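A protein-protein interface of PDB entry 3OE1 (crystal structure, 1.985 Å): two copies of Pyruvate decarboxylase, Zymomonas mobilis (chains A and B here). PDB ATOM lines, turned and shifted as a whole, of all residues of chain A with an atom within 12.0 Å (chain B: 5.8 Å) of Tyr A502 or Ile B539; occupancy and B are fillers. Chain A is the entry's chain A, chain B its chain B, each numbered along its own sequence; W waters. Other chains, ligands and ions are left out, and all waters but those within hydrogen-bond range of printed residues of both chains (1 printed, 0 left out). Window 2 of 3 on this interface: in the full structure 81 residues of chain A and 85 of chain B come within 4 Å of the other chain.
The side-chain hydroxyl (OH) of Tyr A502 is in hydrogen-bond range of the backbone carbonyl oxygen (O) of Asn B466.
O of Ile B539 sits at hydrogen-bond distance from OH of Tyr A502, 3.2 Å away.
The side-chain carboxylate (OD2) of Asp A503 lies within hydrogen-bond range of the side-chain hydroxyl (OH) of Tyr B468, at 3.0 Å.
OD2 of Asp A503 is in hydrogen-bond range of N of Asn B486 (3.1 Å).
The side-chain amide oxygen of Asn B466 sits at hydrogen-bond distance from the backbone NH of Tyr B468 (3.2 Å).
The side-chain amide nitrogen (ND2) of Asn B466 is in hydrogen-bond range of the side-chain amide oxygen (OD1) of Asn B486, 2.8 Å away.
ND2 of Asn B466 sits at hydrogen-bond distance from OE2 of Glu B536 (2.9 Å).
The backbone carbonyl oxygen (O) of Cys B537 is in hydrogen-bond range of the backbone NH (N) of Asn B466 (2.7 Å).
O of Asn B466 lies within hydrogen-bond range of N of Ile B539.
O of Tyr B468 lies within hydrogen-bond range of NH2 of Arg B541.
Among the printed residues, pairs that only touch across the chains: Tyr A502 with Asn B486 (3.5 Å), Phe A496 with Asn B486 (3.5 Å), Tyr A502 with Phe B538 (3.6 Å) and Tyr A502 with Tyr B468 (3.7 Å).
Printed residues of chain B within 4 Å of Phe A496: Asn B486 (3.5 Å).
Asn A497 touches none of the printed residues of chain B.
Gly A500 touches none of the printed residues of chain B.
Of the printed residues of chain B, Asp A503 touches Tyr B468 (3.0 Å) and Asn B486 (3.1 Å).
No residue of chain A comes within 4 Å of Leu B365.
No residue of chain A comes within 4 Å of Val B366.
No residue of chain A comes within 4 Å of Asn B367.
Asn B466 touches one residue of chain A.
Asn B467 touches none of the printed residues of chain A.
Tyr B468 touches just these residues of chain A: Tyr A502 and Asp A503.
Of chain A, only Phe A496, Tyr A502 and Asp A503 come within 4 Å of Asn B486.
Phe B538 touches just one residue of chain A: Tyr A502 (3.6 Å).
Of chain A, only Tyr A502 comes within 4 Å of Ile B539.
No residue of chain A comes within 4 Å of Asp B543.
The nearest residue of chain A that does not touch Ile B539 is Gly A501 (10.5 Å).
Of the 16 printed residues of chain B, 5 touch a printed residue of chain A.
Hydrophobic or aromatic side chains of chain B that line the printed part of chain A: Tyr B468 and Phe B538.
Along chain B the printed residues that touch a printed residue of chain A span positions 466 to 539.
Hydrophobic or aromatic side chains of chain A that line the printed part of chain B: Tyr A502.
Along chain A the printed residues that touch a printed residue of chain B span positions 496 to 503.
Among the printed residues, no Asp or Glu carboxylate lies within 4 Å of a Lys or Arg side-chain nitrogen of the other chain.
No position is printed for both chains.
Of the 8 pairs that touch across the chains among the printed residues, none has its exchanged pair printed and touching as well.
Water W1 lies within hydrogen-bond range of the side-chain carboxylate of Asp A503 (2.5 Å), the backbone carbonyl oxygen of Gly A498 (2.8 Å), the side-chain amide nitrogen of Asn B486 (3.0 Å) and the backbone NH of Tyr A502 (3.2 Å).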
ATOM      1  N   VAL A 454      -2.890 -14.107  -5.924  1.00  0.00           N
ATOM      2  CA  VAL A 454      -2.678 -14.864  -4.694  1.00  0.00           C
ATOM      3  C   VAL A 454      -3.910 -15.722  -4.399  1.00  0.00           C
ATOM      4  O   VAL A 454      -3.804 -16.901  -4.063  1.00  0.00           O
ATOM      5  CB  VAL A 454      -2.400 -13.927  -3.497  1.00  0.00           C
ATOM      6  CG1 VAL A 454      -2.356 -14.717  -2.196  1.00  0.00           C
ATOM      7  CG2 VAL A 454      -1.103 -13.162  -3.706  1.00  0.00           C
ATOM      8  N   ARG A 455      -5.080 -15.120  -4.564  1.00  0.00           N
ATOM      9  CA  ARG A 455      -6.348 -15.795  -4.330  1.00  0.00           C
ATOM     10  C   ARG A 455      -6.500 -17.062  -5.176  1.00  0.00           C
ATOM     11  O   ARG A 455      -6.879 -18.123  -4.667  1.00  0.00           O
ATOM     12  CB  ARG A 455      -7.492 -14.825  -4.623  1.00  0.00           C
ATOM     13  CG  ARG A 455      -8.870 -15.308  -4.203  1.00  0.00           C
ATOM     14  CD  ARG A 455      -9.919 -14.314  -4.675  1.00  0.00           C
ATOM     15  NE  ARG A 455     -11.233 -14.541  -4.083  1.00  0.00           N
ATOM     16  CZ  ARG A 455     -12.260 -13.707  -4.215  1.00  0.00           C
ATOM     17  NH1 ARG A 455     -12.116 -12.587  -4.912  1.00  0.00           N
ATOM     18  NH2 ARG A 455     -13.423 -13.983  -3.642  1.00  0.00           N
ATOM     19  N   LYS A 457      -4.127 -18.633  -6.669  1.00  0.00           N
ATOM     20  CA  LYS A 457      -2.876 -19.391  -6.619  1.00  0.00           C
ATOM     21  C   LYS A 457      -2.122 -19.413  -7.951  1.00  0.00           C
ATOM     22  O   LYS A 457      -1.538 -20.425  -8.336  1.00  0.00           O
ATOM     23  CB  LYS A 457      -3.124 -20.814  -6.100  1.00  0.00           C
ATOM     24  CG  LYS A 457      -3.708 -20.850  -4.696  1.00  0.00           C
ATOM     25  CD  LYS A 457      -3.903 -22.272  -4.210  1.00  0.00           C
ATOM     26  CE  LYS A 457      -4.456 -22.292  -2.798  1.00  0.00           C
ATOM     27  NZ  LYS A 457      -5.785 -21.621  -2.718  1.00  0.00           N
ATOM     28  N   GLU A 494       3.151 -10.102   1.289  1.00  0.00           N
ATOM     29  CA  GLU A 494       2.616 -10.652   2.533  1.00  0.00           C
ATOM     30  C   GLU A 494       1.314  -9.970   2.954  1.00  0.00           C
ATOM     31  O   GLU A 494       0.464 -10.583   3.604  1.00  0.00           O
ATOM     32  CB  GLU A 494       3.648 -10.590   3.664  1.00  0.00           C
ATOM     33  CG  GLU A 494       4.730 -11.646   3.553  1.00  0.00           C
ATOM     34  CD  GLU A 494       4.161 -13.046   3.373  1.00  0.00           C
ATOM     35  OE1 GLU A 494       3.245 -13.429   4.135  1.00  0.00           O
ATOM     36  OE2 GLU A 494       4.631 -13.763   2.462  1.00  0.00           O
ATOM     37  N   VAL A 495       1.161  -8.702   2.592  1.00  0.00           N
ATOM     38  CA  VAL A 495      -0.089  -8.001   2.865  1.00  0.00           C
ATOM     39  C   VAL A 495      -1.234  -8.687   2.126  1.00  0.00           C
ATOM     40  O   VAL A 495      -2.300  -8.922   2.693  1.00  0.00           O
ATOM     41  CB  VAL A 495      -0.023  -6.518   2.469  1.00  0.00           C
ATOM     42  CG1 VAL A 495      -1.413  -5.918   2.438  1.00  0.00           C
ATOM     43  CG2 VAL A 495       0.865  -5.749   3.430  1.00  0.00           C
ATOM     44  N   PHE A 496      -1.002  -9.028   0.862  1.00  0.00           N
ATOM     45  CA  PHE A 496      -2.030  -9.682   0.067  1.00  0.00           C
ATOM     46  C   PHE A 496      -2.278 -11.118   0.536  1.00  0.00           C
ATOM     47  O   PHE A 496      -3.384 -11.631   0.404  1.00  0.00           O
ATOM     48  CB  PHE A 496      -1.677  -9.641  -1.423  1.00  0.00           C
ATOM     49  CG  PHE A 496      -1.701  -8.255  -2.012  1.00  0.00           C
ATOM     50  CD1 PHE A 496      -2.441  -7.246  -1.415  1.00  0.00           C
ATOM     51  CD2 PHE A 496      -0.979  -7.960  -3.157  1.00  0.00           C
ATOM     52  CE1 PHE A 496      -2.462  -5.971  -1.955  1.00  0.00           C
ATOM     53  CE2 PHE A 496      -1.002  -6.685  -3.705  1.00  0.00           C
ATOM     54  CZ  PHE A 496      -1.741  -5.696  -3.105  1.00  0.00           C
ATOM     55  N   ASN A 497      -1.249 -11.764   1.078  1.00  0.00           N
ATOM     56  CA  ASN A 497      -1.429 -13.092   1.651  1.00  0.00           C
ATOM     57  C   ASN A 497      -2.395 -13.050   2.826  1.00  0.00           C
ATOM     58  O   ASN A 497      -3.316 -13.864   2.922  1.00  0.00           O
ATOM     59  CB  ASN A 497      -0.091 -13.694   2.092  1.00  0.00           C
ATOM     60  CG  ASN A 497       0.763 -14.133   0.922  1.00  0.00           C
ATOM     61  OD1 ASN A 497       0.260 -14.330  -0.186  1.00  0.00           O
ATOM     62  ND2 ASN A 497       2.057 -14.300   1.163  1.00  0.00           N
ATOM     63  N   GLY A 498      -2.181 -12.084   3.714  1.00  0.00           N
ATOM     64  CA  GLY A 498      -2.997 -11.948   4.905  1.00  0.00           C
ATOM     65  C   GLY A 498      -2.902 -13.172   5.793  1.00  0.00           C
ATOM     66  O   GLY A 498      -3.846 -13.501   6.507  1.00  0.00           O
ATOM     67  N   ASN A 499      -1.763 -13.854   5.746  1.00  0.00           N
ATOM     68  CA  ASN A 499      -1.547 -15.019   6.597  1.00  0.00           C
ATOM     69  C   ASN A 499      -1.700 -14.655   8.072  1.00  0.00           C
ATOM     70  O   ASN A 499      -1.055 -13.730   8.566  1.00  0.00           O
ATOM     71  CB  ASN A 499      -0.180 -15.656   6.321  1.00  0.00           C
ATOM     72  CG  ASN A 499      -0.118 -16.350   4.963  1.00  0.00           C
ATOM     73  OD1 ASN A 499      -1.098 -16.941   4.506  1.00  0.00           O
ATOM     74  ND2 ASN A 499       1.039 -16.276   4.314  1.00  0.00           N
ATOM     75  N   GLY A 500      -2.566 -15.384   8.767  1.00  0.00           N
ATOM     76  CA  GLY A 500      -2.907 -15.067  10.143  1.00  0.00           C
ATOM     77  C   GLY A 500      -4.272 -14.408  10.230  1.00  0.00           C
ATOM     78  O   GLY A 500      -4.783 -14.150  11.322  1.00  0.00           O
ATOM     79  N   GLY A 501      -4.866 -14.142   9.069  1.00  0.00           N
ATOM     80  CA  GLY A 501      -6.159 -13.484   8.998  1.00  0.00           C
ATOM     81  C   GLY A 501      -7.311 -14.420   8.677  1.00  0.00           C
ATOM     82  O   GLY A 501      -7.304 -15.584   9.076  1.00  0.00           O
ATOM     83  N   TYR A 502      -8.303 -13.900   7.955  1.00  0.00           N
ATOM     84  CA  TYR A 502      -9.509 -14.651   7.606  1.00  0.00           C
ATOM     85  C   TYR A 502      -9.218 -15.787   6.635  1.00  0.00           C
ATOM     86  O   TYR A 502      -9.869 -16.833   6.678  1.00  0.00           O
ATOM     87  CB  TYR A 502     -10.571 -13.728   7.002  1.00  0.00           C
ATOM     88  CG  TYR A 502     -11.243 -12.801   7.991  1.00  0.00           C
ATOM     89  CD1 TYR A 502     -12.318 -13.233   8.759  1.00  0.00           C
ATOM     90  CD2 TYR A 502     -10.819 -11.488   8.141  1.00  0.00           C
ATOM     91  CE1 TYR A 502     -12.938 -12.384   9.662  1.00  0.00           C
ATOM     92  CE2 TYR A 502     -11.432 -10.635   9.039  1.00  0.00           C
ATOM     93  CZ  TYR A 502     -12.490 -11.087   9.797  1.00  0.00           C
ATOM     94  OH  TYR A 502     -13.101 -10.236  10.689  1.00  0.00           O
ATOM     95  N   ASP A 503      -8.253 -15.572   5.749  1.00  0.00           N
ATOM     96  CA  ASP A 503      -7.845 -16.607   4.806  1.00  0.00           C
ATOM     97  C   ASP A 503      -6.326 -16.746   4.744  1.00  0.00           C
ATOM     98  O   ASP A 503      -5.636 -16.539   5.743  1.00  0.00           O
ATOM     99  CB  ASP A 503      -8.459 -16.389   3.411  1.00  0.00           C
ATOM    100  CG  ASP A 503      -8.203 -14.990   2.848  1.00  0.00           C
ATOM    101  OD1 ASP A 503      -7.112 -14.421   3.068  1.00  0.00           O
ATOM    102  OD2 ASP A 503      -9.106 -14.466   2.162  1.00  0.00           O
ATOM    103  N   SER A 504      -5.809 -17.111   3.576  1.00  0.00           N
ATOM    104  CA  SER A 504      -4.376 -17.327   3.426  1.00  0.00           C
ATOM    105  C   SER A 504      -3.904 -17.003   2.014  1.00  0.00           C
ATOM    106  O   SER A 504      -4.708 -16.705   1.135  1.00  0.00           O
ATOM    107  CB  SER A 504      -4.017 -18.772   3.776  1.00  0.00           C
ATOM    108  OG  SER A 504      -4.632 -19.675   2.870  1.00  0.00           O
ATOM    109  N   GLY A 505      -2.595 -17.071   1.804  1.00  0.00           N
ATOM    110  CA  GLY A 505      -2.012 -16.806   0.503  1.00  0.00           C
ATOM    111  C   GLY A 505      -0.569 -17.266   0.459  1.00  0.00           C
ATOM    112  O   GLY A 505       0.101 -17.301   1.494  1.00  0.00           O
ATOM    113  N   ALA A 506      -0.088 -17.623  -0.729  1.00  0.00           N
ATOM    114  CA  ALA A 506       1.282 -18.114  -0.884  1.00  0.00           C
ATOM    115  C   ALA A 506       2.111 -17.278  -1.853  1.00  0.00           C
ATOM    116  O   ALA A 506       3.011 -17.795  -2.513  1.00  0.00           O
ATOM    117  CB  ALA A 506       1.280 -19.567  -1.325  1.00  0.00           C
ATOM    118  N   LEU B 365     -14.580  -7.859  19.272  1.00  0.00           N
ATOM    119  CA  LEU B 365     -15.080  -6.549  18.866  1.00  0.00           C
ATOM    120  C   LEU B 365     -16.375  -6.678  18.072  1.00  0.00           C
ATOM    121  O   LEU B 365     -16.507  -7.564  17.231  1.00  0.00           O
ATOM    122  CB  LEU B 365     -14.032  -5.813  18.030  1.00  0.00           C
ATOM    123  CG  LEU B 365     -14.424  -4.405  17.576  1.00  0.00           C
ATOM    124  CD1 LEU B 365     -14.765  -3.519  18.783  1.00  0.00           C
ATOM    125  CD2 LEU B 365     -13.319  -3.785  16.733  1.00  0.00           C
ATOM    126  N   VAL B 366     -17.333  -5.797  18.345  1.00  0.00           N
ATOM    127  CA  VAL B 366     -18.581  -5.784  17.590  1.00  0.00           C
ATOM    128  C   VAL B 366     -18.814  -4.430  16.934  1.00  0.00           C
ATOM    129  O   VAL B 366     -18.222  -3.424  17.331  1.00  0.00           O
ATOM    130  CB  VAL B 366     -19.796  -6.132  18.470  1.00  0.00           C
ATOM    131  CG1 VAL B 366     -19.650  -7.531  19.042  1.00  0.00           C
ATOM    132  CG2 VAL B 366     -19.962  -5.106  19.579  1.00  0.00           C
ATOM    133  N   ASN B 367     -19.688  -4.410  15.935  1.00  0.00           N
ATOM    134  CA  ASN B 367     -19.992  -3.190  15.194  1.00  0.00           C
ATOM    135  C   ASN B 367     -20.379  -1.994  16.057  1.00  0.00           C
ATOM    136  O   ASN B 367     -19.917  -0.877  15.816  1.00  0.00           O
ATOM    137  CB  ASN B 367     -21.108  -3.438  14.184  1.00  0.00           C
ATOM    138  CG  ASN B 367     -21.497  -2.180  13.450  1.00  0.00           C
ATOM    139  OD1 ASN B 367     -20.643  -1.496  12.889  1.00  0.00           O
ATOM    140  ND2 ASN B 367     -22.781  -1.848  13.472  1.00  0.00           N
ATOM    141  N   ILE B 370     -17.549  -0.205  17.836  1.00  0.00           N
ATOM    142  CA  ILE B 370     -16.760   0.661  16.963  1.00  0.00           C
ATOM    143  C   ILE B 370     -17.440   2.019  16.808  1.00  0.00           C
ATOM    144  O   ILE B 370     -16.816   3.064  16.998  1.00  0.00           O
ATOM    145  CB  ILE B 370     -16.525   0.035  15.576  1.00  0.00           C
ATOM    146  CG1 ILE B 370     -15.795  -1.301  15.709  1.00  0.00           C
ATOM    147  CG2 ILE B 370     -15.739   0.992  14.682  1.00  0.00           C
ATOM    148  CD1 ILE B 370     -15.583  -2.010  14.389  1.00  0.00           C
ATOM    149  N   ILE B 465     -12.963  -1.274   8.312  1.00  0.00           N
ATOM    150  CA  ILE B 465     -13.896  -2.236   8.876  1.00  0.00           C
ATOM    151  C   ILE B 465     -13.744  -3.573   8.165  1.00  0.00           C
ATOM    152  O   ILE B 465     -14.319  -3.797   7.101  1.00  0.00           O
ATOM    153  CB  ILE B 465     -15.363  -1.757   8.789  1.00  0.00           C
ATOM    154  CG1 ILE B 465     -15.512  -0.332   9.335  1.00  0.00           C
ATOM    155  CG2 ILE B 465     -16.277  -2.708   9.536  1.00  0.00           C
ATOM    156  CD1 ILE B 465     -15.027  -0.151  10.763  1.00  0.00           C
ATOM    157  N   ASN B 466     -12.957  -4.460   8.756  1.00  0.00           N
ATOM    158  CA  ASN B 466     -12.714  -5.758   8.154  1.00  0.00           C
ATOM    159  C   ASN B 466     -13.725  -6.799   8.638  1.00  0.00           C
ATOM    160  O   ASN B 466     -13.504  -7.481   9.638  1.00  0.00           O
ATOM    161  CB  ASN B 466     -11.274  -6.209   8.412  1.00  0.00           C
ATOM    162  CG  ASN B 466     -10.898  -7.444   7.621  1.00  0.00           C
ATOM    163  OD1 ASN B 466     -11.715  -7.998   6.885  1.00  0.00           O
ATOM    164  ND2 ASN B 466      -9.652  -7.880   7.766  1.00  0.00           N
ATOM    165  N   ASN B 467     -14.844  -6.890   7.928  1.00  0.00           N
ATOM    166  CA  ASN B 467     -15.836  -7.926   8.188  1.00  0.00           C
ATOM    167  C   ASN B 467     -15.828  -8.961   7.063  1.00  0.00           C
ATOM    168  O   ASN B 467     -16.795  -9.702   6.872  1.00  0.00           O
ATOM    169  CB  ASN B 467     -17.226  -7.310   8.346  1.00  0.00           C
ATOM    170  CG  ASN B 467     -17.681  -6.614   7.095  1.00  0.00           C
ATOM    171  OD1 ASN B 467     -17.037  -6.740   6.061  1.00  0.00           O
ATOM    172  ND2 ASN B 467     -18.778  -5.875   7.175  1.00  0.00           N
ATOM    173  N   TYR B 468     -14.733  -8.976   6.306  1.00  0.00           N
ATOM    174  CA  TYR B 468     -14.457 -10.025   5.329  1.00  0.00           C
ATOM    175  C   TYR B 468     -15.502 -10.126   4.219  1.00  0.00           C
ATOM    176  O   TYR B 468     -16.128 -11.174   4.053  1.00  0.00           O
ATOM    177  CB  TYR B 468     -14.353 -11.374   6.041  1.00  0.00           C
ATOM    178  CG  TYR B 468     -13.651 -12.458   5.254  1.00  0.00           C
ATOM    179  CD1 TYR B 468     -12.656 -12.150   4.334  1.00  0.00           C
ATOM    180  CD2 TYR B 468     -13.986 -13.795   5.435  1.00  0.00           C
ATOM    181  CE1 TYR B 468     -12.011 -13.148   3.617  1.00  0.00           C
ATOM    182  CE2 TYR B 468     -13.352 -14.794   4.725  1.00  0.00           C
ATOM    183  CZ  TYR B 468     -12.366 -14.468   3.817  1.00  0.00           C
ATOM    184  OH  TYR B 468     -11.736 -15.466   3.112  1.00  0.00           O
ATOM    185  N   ASN B 486      -9.028 -11.420   1.644  1.00  0.00           N
ATOM    186  CA  ASN B 486      -8.632 -10.617   2.788  1.00  0.00           C
ATOM    187  C   ASN B 486      -7.174 -10.177   2.690  1.00  0.00           C
ATOM    188  O   ASN B 486      -6.322 -10.924   2.211  1.00  0.00           O
ATOM    189  CB  ASN B 486      -8.846 -11.417   4.070  1.00  0.00           C
ATOM    190  CG  ASN B 486      -8.596 -10.600   5.312  1.00  0.00           C
ATOM    191  OD1 ASN B 486      -9.342  -9.663   5.608  1.00  0.00           O
ATOM    192  ND2 ASN B 486      -7.556 -10.959   6.062  1.00  0.00           N
ATOM    193  N   GLU B 536      -7.273  -1.492  11.656  1.00  0.00           N
ATOM    194  CA  GLU B 536      -7.999  -2.623  11.100  1.00  0.00           C
ATOM    195  C   GLU B 536      -8.905  -3.219  12.161  1.00  0.00           C
ATOM    196  O   GLU B 536      -8.430  -3.838  13.111  1.00  0.00           O
ATOM    197  CB  GLU B 536      -7.024  -3.684  10.592  1.00  0.00           C
ATOM    198  CG  GLU B 536      -7.692  -4.877   9.925  1.00  0.00           C
ATOM    199  CD  GLU B 536      -6.691  -5.869   9.358  1.00  0.00           C
ATOM    200  OE1 GLU B 536      -5.471  -5.690   9.574  1.00  0.00           O
ATOM    201  OE2 GLU B 536      -7.128  -6.835   8.691  1.00  0.00           O
ATOM    202  N   CYS B 537     -10.209  -3.023  11.996  1.00  0.00           N
ATOM    203  CA  CYS B 537     -11.194  -3.513  12.952  1.00  0.00           C
ATOM    204  C   CYS B 537     -11.818  -4.828  12.479  1.00  0.00           C
ATOM    205  O   CYS B 537     -12.383  -4.904  11.385  1.00  0.00           O
ATOM    206  CB  CYS B 537     -12.274  -2.452  13.189  1.00  0.00           C
ATOM    207  SG  CYS B 537     -11.632  -0.861  13.811  1.00  0.00           S
ATOM    208  N   PHE B 538     -11.708  -5.860  13.309  1.00  0.00           N
ATOM    209  CA  PHE B 538     -12.232  -7.178  12.968  1.00  0.00           C
ATOM    210  C   PHE B 538     -13.602  -7.405  13.595  1.00  0.00           C
ATOM    211  O   PHE B 538     -13.735  -7.435  14.820  1.00  0.00           O
ATOM    212  CB  PHE B 538     -11.274  -8.278  13.439  1.00  0.00           C
ATOM    213  CG  PHE B 538      -9.910  -8.209  12.817  1.00  0.00           C
ATOM    214  CD1 PHE B 538      -8.942  -7.358  13.329  1.00  0.00           C
ATOM    215  CD2 PHE B 538      -9.591  -9.000  11.726  1.00  0.00           C
ATOM    216  CE1 PHE B 538      -7.683  -7.291  12.759  1.00  0.00           C
ATOM    217  CE2 PHE B 538      -8.333  -8.938  11.151  1.00  0.00           C
ATOM    218  CZ  PHE B 538      -7.379  -8.081  11.669  1.00  0.00           C
ATOM    219  N   ILE B 539     -14.612  -7.571  12.744  1.00  0.00           N
ATOM    220  CA  ILE B 539     -15.972  -7.865  13.178  1.00  0.00           C
ATOM    221  C   ILE B 539     -16.609  -8.898  12.249  1.00  0.00           C
ATOM    222  O   ILE B 539     -16.094  -9.164  11.162  1.00  0.00           O
ATOM    223  CB  ILE B 539     -16.856  -6.604  13.173  1.00  0.00           C
ATOM    224  CG1 ILE B 539     -17.065  -6.110  11.740  1.00  0.00           C
ATOM    225  CG2 ILE B 539     -16.245  -5.513  14.047  1.00  0.00           C
ATOM    226  CD1 ILE B 539     -18.131  -5.045  11.615  1.00  0.00           C
ATOM    227  N   GLY B 540     -17.737  -9.467  12.670  1.00  0.00           N
ATOM    228  CA  GLY B 540     -18.419 -10.483  11.883  1.00  0.00           C
ATOM    229  C   GLY B 540     -19.174  -9.941  10.679  1.00  0.00           C
ATOM    230  O   GLY B 540     -19.638  -8.805  10.688  1.00  0.00           O
ATOM    231  N   ARG B 541     -19.295 -10.752   9.634  1.00  0.00           N
ATOM    232  CA  ARG B 541     -20.057 -10.355   8.455  1.00  0.00           C
ATOM    233  C   ARG B 541     -21.487  -9.960   8.815  1.00  0.00           C
ATOM    234  O   ARG B 541     -22.013  -8.965   8.311  1.00  0.00           O
ATOM    235  CB  ARG B 541     -20.093 -11.480   7.423  1.00  0.00           C
ATOM    236  CG  ARG B 541     -21.255 -11.358   6.450  1.00  0.00           C
ATOM    237  CD  ARG B 541     -21.094 -12.270   5.244  1.00  0.00           C
ATOM    238  NE  ARG B 541     -19.907 -11.937   4.465  1.00  0.00           N
ATOM    239  CZ  ARG B 541     -19.557 -12.546   3.337  1.00  0.00           C
ATOM    240  NH1 ARG B 541     -20.309 -13.522   2.846  1.00  0.00           N
ATOM    241  NH2 ARG B 541     -18.453 -12.178   2.699  1.00  0.00           N
ATOM    242  N   ASP B 543     -22.678  -9.058  11.761  1.00  0.00           N
ATOM    243  CA  ASP B 543     -22.809  -8.056  12.815  1.00  0.00           C
ATOM    244  C   ASP B 543     -22.841  -6.638  12.264  1.00  0.00           C
ATOM    245  O   ASP B 543     -21.841  -5.920  12.308  1.00  0.00           O
ATOM    246  CB  ASP B 543     -21.687  -8.202  13.842  1.00  0.00           C
ATOM    247  CG  ASP B 543     -21.850  -7.260  15.016  1.00  0.00           C
ATOM    248  OD1 ASP B 543     -22.989  -6.810  15.270  1.00  0.00           O
ATOM    249  OD2 ASP B 543     -20.837  -6.975  15.691  1.00  0.00           O
HETATM  250  O   HOH W   1      -6.446 -13.696   5.385  1.00  0.00           O
